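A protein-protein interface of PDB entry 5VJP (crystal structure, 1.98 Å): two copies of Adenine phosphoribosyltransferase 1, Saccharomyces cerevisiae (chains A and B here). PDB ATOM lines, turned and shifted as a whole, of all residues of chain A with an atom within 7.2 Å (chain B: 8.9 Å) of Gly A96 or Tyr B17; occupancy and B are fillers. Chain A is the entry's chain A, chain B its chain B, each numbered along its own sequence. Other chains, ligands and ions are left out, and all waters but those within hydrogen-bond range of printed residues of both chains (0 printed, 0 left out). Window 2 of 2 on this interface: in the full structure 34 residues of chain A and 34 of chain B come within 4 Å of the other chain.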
ATOM      1  N   LEU A  94      16.325  13.034  -2.440  1.00  0.00           N
ATOM      2  CA  LEU A  94      15.573  13.218  -1.194  1.00  0.00           C
ATOM      3  C   LEU A  94      15.877  12.106  -0.202  1.00  0.00           C
ATOM      4  O   LEU A  94      15.849  10.933  -0.573  1.00  0.00           O
ATOM      5  CB  LEU A  94      14.065  13.269  -1.461  1.00  0.00           C
ATOM      6  CG  LEU A  94      13.589  14.541  -2.166  1.00  0.00           C
ATOM      7  CD1 LEU A  94      12.228  14.332  -2.807  1.00  0.00           C
ATOM      8  CD2 LEU A  94      13.551  15.710  -1.200  1.00  0.00           C
ATOM      9  N   PRO A  95      16.155  12.462   1.066  1.00  0.00           N
ATOM     10  CA  PRO A  95      16.384  11.449   2.090  1.00  0.00           C
ATOM     11  C   PRO A  95      15.067  10.929   2.654  1.00  0.00           C
ATOM     12  O   PRO A  95      14.026  11.570   2.480  1.00  0.00           O
ATOM     13  CB  PRO A  95      17.131  12.229   3.163  1.00  0.00           C
ATOM     14  CG  PRO A  95      16.493  13.583   3.107  1.00  0.00           C
ATOM     15  CD  PRO A  95      16.206  13.821   1.644  1.00  0.00           C
ATOM     16  N   GLY A  96      15.127   9.790   3.340  1.00  0.00           N
ATOM     17  CA  GLY A  96      13.952   9.194   3.970  1.00  0.00           C
ATOM     18  C   GLY A  96      13.078   8.447   2.986  1.00  0.00           C
ATOM     19  O   GLY A  96      13.445   8.281   1.823  1.00  0.00           O
ATOM     20  N   GLU A  97      11.916   7.998   3.460  1.00  0.00           N
ATOM     21  CA  GLU A  97      10.991   7.215   2.635  1.00  0.00           C
ATOM     22  C   GLU A  97      10.282   8.139   1.646  1.00  0.00           C
ATOM     23  O   GLU A  97       9.683   9.136   2.048  1.00  0.00           O
ATOM     24  CB  GLU A  97       9.951   6.489   3.495  1.00  0.00           C
ATOM     25  CG  GLU A  97      10.512   5.507   4.516  1.00  0.00           C
ATOM     26  CD  GLU A  97      11.196   4.308   3.884  1.00  0.00           C
ATOM     27  OE1 GLU A  97      12.354   4.451   3.437  1.00  0.00           O
ATOM     28  OE2 GLU A  97      10.588   3.215   3.847  1.00  0.00           O
ATOM     29  N   CYS A  98      10.359   7.790   0.363  1.00  0.00           N
ATOM     30  CA  CYS A  98       9.765   8.578  -0.709  1.00  0.00           C
ATOM     31  C   CYS A  98       8.790   7.755  -1.542  1.00  0.00           C
ATOM     32  O   CYS A  98       8.928   6.535  -1.636  1.00  0.00           O
ATOM     33  CB  CYS A  98      10.862   9.102  -1.634  1.00  0.00           C
ATOM     34  SG  CYS A  98      12.015  10.249  -0.862  1.00  0.00           S
ATOM     35  N   PHE A  99       7.807   8.435  -2.133  1.00  0.00           N
ATOM     36  CA  PHE A  99       7.041   7.884  -3.249  1.00  0.00           C
ATOM     37  C   PHE A  99       7.792   8.170  -4.538  1.00  0.00           C
ATOM     38  O   PHE A  99       8.586   9.111  -4.613  1.00  0.00           O
ATOM     39  CB  PHE A  99       5.647   8.494  -3.342  1.00  0.00           C
ATOM     40  CG  PHE A  99       4.733   8.093  -2.226  1.00  0.00           C
ATOM     41  CD1 PHE A  99       4.393   6.756  -2.030  1.00  0.00           C
ATOM     42  CD2 PHE A  99       4.186   9.051  -1.384  1.00  0.00           C
ATOM     43  CE1 PHE A  99       3.541   6.388  -1.001  1.00  0.00           C
ATOM     44  CE2 PHE A  99       3.335   8.689  -0.355  1.00  0.00           C
ATOM     45  CZ  PHE A  99       3.015   7.355  -0.160  1.00  0.00           C
ATOM     46  N   GLU A 113      10.744  11.904  -7.295  1.00  0.00           N
ATOM     47  CA  GLU A 113      10.371  11.483  -5.946  1.00  0.00           C
ATOM     48  C   GLU A 113       9.795  12.631  -5.117  1.00  0.00           C
ATOM     49  O   GLU A 113      10.057  13.805  -5.392  1.00  0.00           O
ATOM     50  CB  GLU A 113      11.580  10.888  -5.215  1.00  0.00           C
ATOM     51  CG  GLU A 113      12.026   9.537  -5.742  1.00  0.00           C
ATOM     52  CD  GLU A 113      13.211   8.965  -4.986  1.00  0.00           C
ATOM     53  OE1 GLU A 113      14.200   9.699  -4.771  1.00  0.00           O
ATOM     54  OE2 GLU A 113      13.155   7.771  -4.619  1.00  0.00           O
ATOM     55  N   ILE A 114       8.997  12.266  -4.115  1.00  0.00           N
ATOM     56  CA  ILE A 114       8.518  13.189  -3.088  1.00  0.00           C
ATOM     57  C   ILE A 114       8.609  12.462  -1.744  1.00  0.00           C
ATOM     58  O   ILE A 114       8.501  11.242  -1.695  1.00  0.00           O
ATOM     59  CB  ILE A 114       7.073  13.684  -3.386  1.00  0.00           C
ATOM     60  CG1 ILE A 114       6.826  15.074  -2.796  1.00  0.00           C
ATOM     61  CG2 ILE A 114       6.000  12.693  -2.907  1.00  0.00           C
ATOM     62  CD1 ILE A 114       5.593  15.755  -3.359  1.00  0.00           C
ATOM     63  N   GLN A 115       8.809  13.211  -0.665  1.00  0.00           N
ATOM     64  CA  GLN A 115       8.913  12.625   0.674  1.00  0.00           C
ATOM     65  C   GLN A 115       7.532  12.277   1.228  1.00  0.00           C
ATOM     66  O   GLN A 115       6.647  13.132   1.290  1.00  0.00           O
ATOM     67  CB  GLN A 115       9.649  13.573   1.627  1.00  0.00           C
ATOM     68  CG  GLN A 115      11.157  13.602   1.370  1.00  0.00           C
ATOM     69  CD  GLN A 115      11.852  14.742   2.072  1.00  0.00           C
ATOM     70  OE1 GLN A 115      11.451  15.882   1.948  1.00  0.00           O
ATOM     71  NE2 GLN A 115      12.916  14.440   2.787  1.00  0.00           N
ATOM     72  N   LYS A 116       7.373  11.017   1.636  1.00  0.00           N
ATOM     73  CA  LYS A 116       6.096  10.493   2.152  1.00  0.00           C
ATOM     74  C   LYS A 116       5.524  11.312   3.311  1.00  0.00           C
ATOM     75  O   LYS A 116       4.307  11.462   3.420  1.00  0.00           O
ATOM     76  CB  LYS A 116       6.249   9.030   2.600  1.00  0.00           C
ATOM     77  CG  LYS A 116       6.478   8.044   1.467  1.00  0.00           C
ATOM     78  CD  LYS A 116       6.328   6.606   1.936  1.00  0.00           C
ATOM     79  CE  LYS A 116       6.510   5.617   0.794  1.00  0.00           C
ATOM     80  NZ  LYS A 116       7.140   4.332   1.205  1.00  0.00           N
ATOM     81  N   ASN A 117       6.404  11.839   4.161  1.00  0.00           N
ATOM     82  CA  ASN A 117       5.989  12.607   5.346  1.00  0.00           C
ATOM     83  C   ASN A 117       5.697  14.096   5.097  1.00  0.00           C
ATOM     84  O   ASN A 117       5.324  14.808   6.034  1.00  0.00           O
ATOM     85  CB  ASN A 117       7.032  12.449   6.474  1.00  0.00           C
ATOM     86  CG  ASN A 117       8.331  13.205   6.209  1.00  0.00           C
ATOM     87  OD1 ASN A 117       8.697  13.479   5.063  1.00  0.00           O
ATOM     88  ND2 ASN A 117       9.042  13.534   7.281  1.00  0.00           N
ATOM     89  N   ALA B  13      13.803  21.943  13.757  1.00  0.00           N
ATOM     90  CA  ALA B  13      13.053  21.516  12.572  1.00  0.00           C
ATOM     91  C   ALA B  13      13.842  20.583  11.632  1.00  0.00           C
ATOM     92  O   ALA B  13      13.237  19.853  10.846  1.00  0.00           O
ATOM     93  CB  ALA B  13      12.546  22.733  11.813  1.00  0.00           C
ATOM     94  N   LEU B  14      15.172  20.599  11.710  1.00  0.00           N
ATOM     95  CA  LEU B  14      15.998  19.699  10.884  1.00  0.00           C
ATOM     96  C   LEU B  14      15.700  18.230  11.204  1.00  0.00           C
ATOM     97  O   LEU B  14      15.385  17.895  12.348  1.00  0.00           O
ATOM     98  CB  LEU B  14      17.497  19.963  11.087  1.00  0.00           C
ATOM     99  CG  LEU B  14      18.080  21.360  10.835  1.00  0.00           C
ATOM    100  CD1 LEU B  14      19.597  21.303  10.977  1.00  0.00           C
ATOM    101  CD2 LEU B  14      17.679  21.896   9.468  1.00  0.00           C
ATOM    102  N   HIS B  15      15.794  17.374  10.188  1.00  0.00           N
ATOM    103  CA  HIS B  15      15.547  15.936  10.316  1.00  0.00           C
ATOM    104  C   HIS B  15      16.835  15.204   9.929  1.00  0.00           C
ATOM    105  O   HIS B  15      17.348  15.388   8.822  1.00  0.00           O
ATOM    106  CB  HIS B  15      14.383  15.526   9.396  1.00  0.00           C
ATOM    107  CG  HIS B  15      13.744  14.212   9.745  1.00  0.00           C
ATOM    108  ND1 HIS B  15      12.383  14.006   9.664  1.00  0.00           N
ATOM    109  CD2 HIS B  15      14.275  13.038  10.163  1.00  0.00           C
ATOM    110  CE1 HIS B  15      12.103  12.763  10.017  1.00  0.00           C
ATOM    111  NE2 HIS B  15      13.234  12.155  10.326  1.00  0.00           N
ATOM    112  N   GLN B  16      17.336  14.370  10.831  1.00  0.00           N
ATOM    113  CA  GLN B  16      18.590  13.633  10.624  1.00  0.00           C
ATOM    114  C   GLN B  16      18.276  12.307   9.929  1.00  0.00           C
ATOM    115  O   GLN B  16      17.370  11.594  10.354  1.00  0.00           O
ATOM    116  CB  GLN B  16      19.299  13.330  11.963  1.00  0.00           C
ATOM    117  CG  GLN B  16      19.106  14.316  13.122  1.00  0.00           C
ATOM    118  CD  GLN B  16      19.546  15.730  12.802  1.00  0.00           C
ATOM    119  OE1 GLN B  16      20.319  15.955  11.874  1.00  0.00           O
ATOM    120  NE2 GLN B  16      19.067  16.691  13.588  1.00  0.00           N
ATOM    121  N   TYR B  17      19.024  11.979   8.876  1.00  0.00           N
ATOM    122  CA  TYR B  17      18.859  10.705   8.155  1.00  0.00           C
ATOM    123  C   TYR B  17      20.181   9.939   8.096  1.00  0.00           C
ATOM    124  O   TYR B  17      21.018  10.215   7.234  1.00  0.00           O
ATOM    125  CB  TYR B  17      18.306  10.939   6.748  1.00  0.00           C
ATOM    126  CG  TYR B  17      16.875  11.416   6.744  1.00  0.00           C
ATOM    127  CD1 TYR B  17      15.824  10.509   6.799  1.00  0.00           C
ATOM    128  CD2 TYR B  17      16.570  12.781   6.685  1.00  0.00           C
ATOM    129  CE1 TYR B  17      14.506  10.939   6.796  1.00  0.00           C
ATOM    130  CE2 TYR B  17      15.256  13.219   6.680  1.00  0.00           C
ATOM    131  CZ  TYR B  17      14.227  12.295   6.735  1.00  0.00           C
ATOM    132  OH  TYR B  17      12.919  12.722   6.736  1.00  0.00           O
ATOM    133  N   PRO B  18      20.380   8.979   9.025  1.00  0.00           N
ATOM    134  CA  PRO B  18      21.602   8.168   9.026  1.00  0.00           C
ATOM    135  C   PRO B  18      21.809   7.394   7.731  1.00  0.00           C
ATOM    136  O   PRO B  18      20.850   6.870   7.172  1.00  0.00           O
ATOM    137  CB  PRO B  18      21.382   7.181  10.182  1.00  0.00           C
ATOM    138  CG  PRO B  18      20.341   7.800  11.039  1.00  0.00           C
ATOM    139  CD  PRO B  18      19.474   8.607  10.127  1.00  0.00           C
ATOM    140  N   ASN B  19      23.054   7.351   7.267  1.00  0.00           N
ATOM    141  CA  ASN B  19      23.462   6.522   6.128  1.00  0.00           C
ATOM    142  C   ASN B  19      22.717   6.845   4.830  1.00  0.00           C
ATOM    143  O   ASN B  19      22.299   5.943   4.098  1.00  0.00           O
ATOM    144  CB  ASN B  19      23.339   5.038   6.487  1.00  0.00           C
ATOM    145  CG  ASN B  19      24.069   4.701   7.769  1.00  0.00           C
ATOM    146  OD1 ASN B  19      25.288   4.864   7.853  1.00  0.00           O
ATOM    147  ND2 ASN B  19      23.328   4.247   8.779  1.00  0.00           N
ATOM    148  N   PHE B  20      22.547   8.141   4.570  1.00  0.00           N
ATOM    149  CA  PHE B  20      22.080   8.638   3.280  1.00  0.00           C
ATOM    150  C   PHE B  20      23.013   9.777   2.844  1.00  0.00           C
ATOM    151  O   PHE B  20      23.351  10.619   3.678  1.00  0.00           O
ATOM    152  CB  PHE B  20      20.637   9.136   3.376  1.00  0.00           C
ATOM    153  CG  PHE B  20      20.025   9.448   2.039  1.00  0.00           C
ATOM    154  CD1 PHE B  20      19.438   8.443   1.279  1.00  0.00           C
ATOM    155  CD2 PHE B  20      20.067  10.739   1.522  1.00  0.00           C
ATOM    156  CE1 PHE B  20      18.891   8.723   0.035  1.00  0.00           C
ATOM    157  CE2 PHE B  20      19.521  11.028   0.283  1.00  0.00           C
ATOM    158  CZ  PHE B  20      18.932  10.020  -0.464  1.00  0.00           C
ATOM    159  N   PRO B  21      23.444   9.833   1.578  1.00  0.00           N
ATOM    160  CA  PRO B  21      23.103   8.880   0.502  1.00  0.00           C
ATOM    161  C   PRO B  21      23.794   7.504   0.573  1.00  0.00           C
ATOM    162  O   PRO B  21      23.337   6.571  -0.088  1.00  0.00           O
ATOM    163  CB  PRO B  21      23.549   9.622  -0.766  1.00  0.00           C
ATOM    164  CG  PRO B  21      24.633  10.536  -0.307  1.00  0.00           C
ATOM    165  CD  PRO B  21      24.240  10.969   1.078  1.00  0.00           C
ATOM    166  N   SER B  22      24.871   7.383   1.347  1.00  0.00           N
ATOM    167  CA  SER B  22      25.583   6.110   1.488  1.00  0.00           C
ATOM    168  C   SER B  22      26.009   5.878   2.933  1.00  0.00           C
ATOM    169  O   SER B  22      25.798   6.738   3.789  1.00  0.00           O
ATOM    170  CB  SER B  22      26.789   6.069   0.542  1.00  0.00           C
ATOM    171  OG  SER B  22      27.739   7.067   0.869  1.00  0.00           O
ATOM    172  N   GLU B  23      26.581   4.698   3.191  1.00  0.00           N
ATOM    173  CA  GLU B  23      27.046   4.294   4.527  1.00  0.00           C
ATOM    174  C   GLU B  23      27.989   5.333   5.123  1.00  0.00           C
ATOM    175  O   GLU B  23      28.896   5.806   4.444  1.00  0.00           O
ATOM    176  CB  GLU B  23      27.766   2.939   4.444  1.00  0.00           C
ATOM    177  CG  GLU B  23      28.178   2.319   5.781  1.00  0.00           C
ATOM    178  CD  GLU B  23      27.019   1.771   6.601  1.00  0.00           C
ATOM    179  OE1 GLU B  23      25.860   1.801   6.130  1.00  0.00           O
ATOM    180  OE2 GLU B  23      27.283   1.306   7.730  1.00  0.00           O
ATOM    181  N   GLY B  24      27.746   5.700   6.381  1.00  0.00           N
ATOM    182  CA  GLY B  24      28.615   6.625   7.117  1.00  0.00           C
ATOM    183  C   GLY B  24      28.215   8.091   7.076  1.00  0.00           C
ATOM    184  O   GLY B  24      28.508   8.831   8.019  1.00  0.00           O
ATOM    185  N   ILE B  25      27.546   8.516   6.000  1.00  0.00           N
ATOM    186  CA  ILE B  25      27.176   9.912   5.817  1.00  0.00           C
ATOM    187  C   ILE B  25      25.902  10.202   6.608  1.00  0.00           C
ATOM    188  O   ILE B  25      24.926   9.458   6.522  1.00  0.00           O
ATOM    189  CB  ILE B  25      26.974  10.259   4.320  1.00  0.00           C
ATOM    190  CG1 ILE B  25      28.258   9.964   3.520  1.00  0.00           C
ATOM    191  CG2 ILE B  25      26.580  11.726   4.159  1.00  0.00           C
ATOM    192  CD1 ILE B  25      28.082   9.961   2.012  1.00  0.00           C
ATOM    193  N   LEU B  26      25.927  11.280   7.392  1.00  0.00           N
ATOM    194  CA  LEU B  26      24.750  11.755   8.118  1.00  0.00           C
ATOM    195  C   LEU B  26      24.131  12.918   7.342  1.00  0.00           C
ATOM    196  O   LEU B  26      24.742  13.985   7.232  1.00  0.00           O
ATOM    197  CB  LEU B  26      25.138  12.199   9.530  1.00  0.00           C
ATOM    198  CG  LEU B  26      23.989  12.642  10.440  1.00  0.00           C
ATOM    199  CD1 LEU B  26      23.064  11.477  10.747  1.00  0.00           C
ATOM    200  CD2 LEU B  26      24.537  13.252  11.722  1.00  0.00           C
ATOM    201  N   PHE B  27      22.925  12.708   6.808  1.00  0.00           N
ATOM    202  CA  PHE B  27      22.241  13.720   5.996  1.00  0.00           C
ATOM    203  C   PHE B  27      21.434  14.652   6.898  1.00  0.00           C
ATOM    204  O   PHE B  27      20.586  14.202   7.668  1.00  0.00           O
ATOM    205  CB  PHE B  27      21.319  13.055   4.970  1.00  0.00           C
ATOM    206  CG  PHE B  27      20.967  13.929   3.798  1.00  0.00           C
ATOM    207  CD1 PHE B  27      19.871  14.799   3.857  1.00  0.00           C
ATOM    208  CD2 PHE B  27      21.723  13.885   2.634  1.00  0.00           C
ATOM    209  CE1 PHE B  27      19.554  15.605   2.777  1.00  0.00           C
ATOM    210  CE2 PHE B  27      21.403  14.686   1.547  1.00  0.00           C
ATOM    211  CZ  PHE B  27      20.318  15.547   1.616  1.00  0.00           C
ATOM    212  N   GLU B  28      21.726  15.946   6.808  1.00  0.00           N
ATOM    213  CA  GLU B  28      20.954  16.988   7.477  1.00  0.00           C
ATOM    214  C   GLU B  28      19.907  17.483   6.476  1.00  0.00           C
ATOM    215  O   GLU B  28      20.254  18.155   5.497  1.00  0.00           O
ATOM    216  CB  GLU B  28      21.871  18.152   7.867  1.00  0.00           C
ATOM    217  CG  GLU B  28      22.960  17.825   8.881  1.00  0.00           C
ATOM    218  CD  GLU B  28      22.420  17.557  10.271  1.00  0.00           C
ATOM    219  OE1 GLU B  28      21.310  18.038  10.596  1.00  0.00           O
ATOM    220  OE2 GLU B  28      23.114  16.867  11.049  1.00  0.00           O
ATOM    221  N   ASP B  29      18.641  17.136   6.712  1.00  0.00           N
ATOM    222  CA  ASP B  29      17.551  17.549   5.832  1.00  0.00           C
ATOM    223  C   ASP B  29      16.924  18.835   6.372  1.00  0.00           C
ATOM    224  O   ASP B  29      16.258  18.818   7.399  1.00  0.00           O
ATOM    225  CB  ASP B  29      16.492  16.439   5.721  1.00  0.00           C
ATOM    226  CG  ASP B  29      15.425  16.726   4.658  1.00  0.00           C
ATOM    227  OD1 ASP B  29      15.666  17.545   3.740  1.00  0.00           O
ATOM    228  OD2 ASP B  29      14.338  16.111   4.740  1.00  0.00           O
ATOM    229  N   PHE B  30      17.163  19.945   5.680  1.00  0.00           N
ATOM    230  CA  PHE B  30      16.514  21.236   5.998  1.00  0.00           C
ATOM    231  C   PHE B  30      15.134  21.458   5.339  1.00  0.00           C
ATOM    232  O   PHE B  30      14.488  22.480   5.586  1.00  0.00           O
ATOM    233  CB  PHE B  30      17.489  22.418   5.759  1.00  0.00           C
ATOM    234  CG  PHE B  30      17.634  22.874   4.312  1.00  0.00           C
ATOM    235  CD1 PHE B  30      17.422  22.027   3.212  1.00  0.00           C
ATOM    236  CD2 PHE B  30      18.049  24.179   4.061  1.00  0.00           C
ATOM    237  CE1 PHE B  30      17.577  22.486   1.914  1.00  0.00           C
ATOM    238  CE2 PHE B  30      18.217  24.640   2.756  1.00  0.00           C
ATOM    239  CZ  PHE B  30      17.981  23.791   1.681  1.00  0.00           C
ATOM    240  N   LEU B  31      14.663  20.493   4.546  1.00  0.00           N
ATOM    241  CA  LEU B  31      13.379  20.633   3.845  1.00  0.00           C
ATOM    242  C   LEU B  31      12.144  20.841   4.726  1.00  0.00           C
ATOM    243  O   LEU B  31      11.208  21.507   4.292  1.00  0.00           O
ATOM    244  CB  LEU B  31      13.140  19.469   2.876  1.00  0.00           C
ATOM    245  CG  LEU B  31      14.090  19.486   1.675  1.00  0.00           C
ATOM    246  CD1 LEU B  31      13.978  18.195   0.880  1.00  0.00           C
ATOM    247  CD2 LEU B  31      13.850  20.697   0.786  1.00  0.00           C
ATOM    248  N   PRO B  32      12.137  20.292   5.962  1.00  0.00           N
ATOM    249  CA  PRO B  32      11.022  20.600   6.868  1.00  0.00           C
ATOM    250  C   PRO B  32      10.807  22.081   7.199  1.00  0.00           C
ATOM    251  O   PRO B  32       9.694  22.459   7.542  1.00  0.00           O
ATOM    252  CB  PRO B  32      11.383  19.818   8.134  1.00  0.00           C
ATOM    253  CG  PRO B  32      12.133  18.637   7.614  1.00  0.00           C
ATOM    254  CD  PRO B  32      12.959  19.181   6.486  1.00  0.00           C
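NE2 of Gln A115 sits at hydrogen-bond distance from OD2 of Asp B29 (2.9 Å).
O of Leu A94 touches CZ of Phe B20, at 3.2 Å. CD1 of Leu B31 touches CD2 of Leu A94 (3.3 Å). Pro A95 touches Tyr B17. Phe B20 touches Pro A95. CG of Pro A95 touches CD1 of Phe B27 (3.7 Å). CG of Pro A95 touches CG of Asp B29, at 3.7 Å. Gly A96 touches Tyr B17 (CA to CE1, 3.4 Å). Gln A115 touches Leu B31 (OE1 to CD1, 3.6 Å). ND2 of Asn A117 touches OH of Tyr B17 (3.998 Å).
SG of Cys A98 is in hydrogen-bond range of O of Gly A96 (3.6 Å). A ring nitrogen (ND1) of His B15 sits at hydrogen-bond distance from the side-chain hydroxyl (OH) of Tyr B17, at 3.2 Å. N of Asp B29 sits at hydrogen-bond distance from O of His B15, 3.0 Å away. The backbone NH (N) of Tyr B17 lies within hydrogen-bond range of the backbone carbonyl oxygen (O) of Phe B27 (3.0 Å). The backbone NH (N) of Phe B20 lies within hydrogen-bond range of the backbone carbonyl oxygen (O) of Ile B25 (3.3 Å). OD1 of Asp B29 is in hydrogen-bond range of N of Leu B31.
Printed residues of chain B within 4 Å of Leu A94: Phe B20 and Leu B31. Of chain B, only Tyr B17, Phe B20, Phe B27 and Asp B29 come within 4 Å of Pro A95. Of the printed residues of chain B, Gly A96 touches Tyr B17. Of the printed residues of chain A, Tyr B17 touches Pro A95, Gly A96 and Asn A117. Printed residues of chain A within 4 Å of Phe B20: Leu A94 (3.2 Å) and Pro A95 (3.6 Å). Printed residues of chain A within 4 Å of Asp B29: Pro A95 (3.7 Å) and Gln A115 (2.9 Å). Of the printed residues of chain A, Leu B31 touches Leu A94 and Gln A115. The nearest residue of chain B that does not touch Gly A96 is Phe B20 (5.0 Å). The nearest printed residue of chain A that does not touch Phe B20 is Gly A96 (5.0 Å).
No position is printed for both chains.
Hydrophobic or aromatic side chains of chain B that line the printed part of chain A: Tyr B17, Phe B20, Phe B27 and Leu B31. Among the printed residues, 10 pairs touch across the chains. Among the printed residues, no Asp or Glu carboxylate lies within 4 Å of a Lys or Arg side-chain nitrogen of the other chain.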
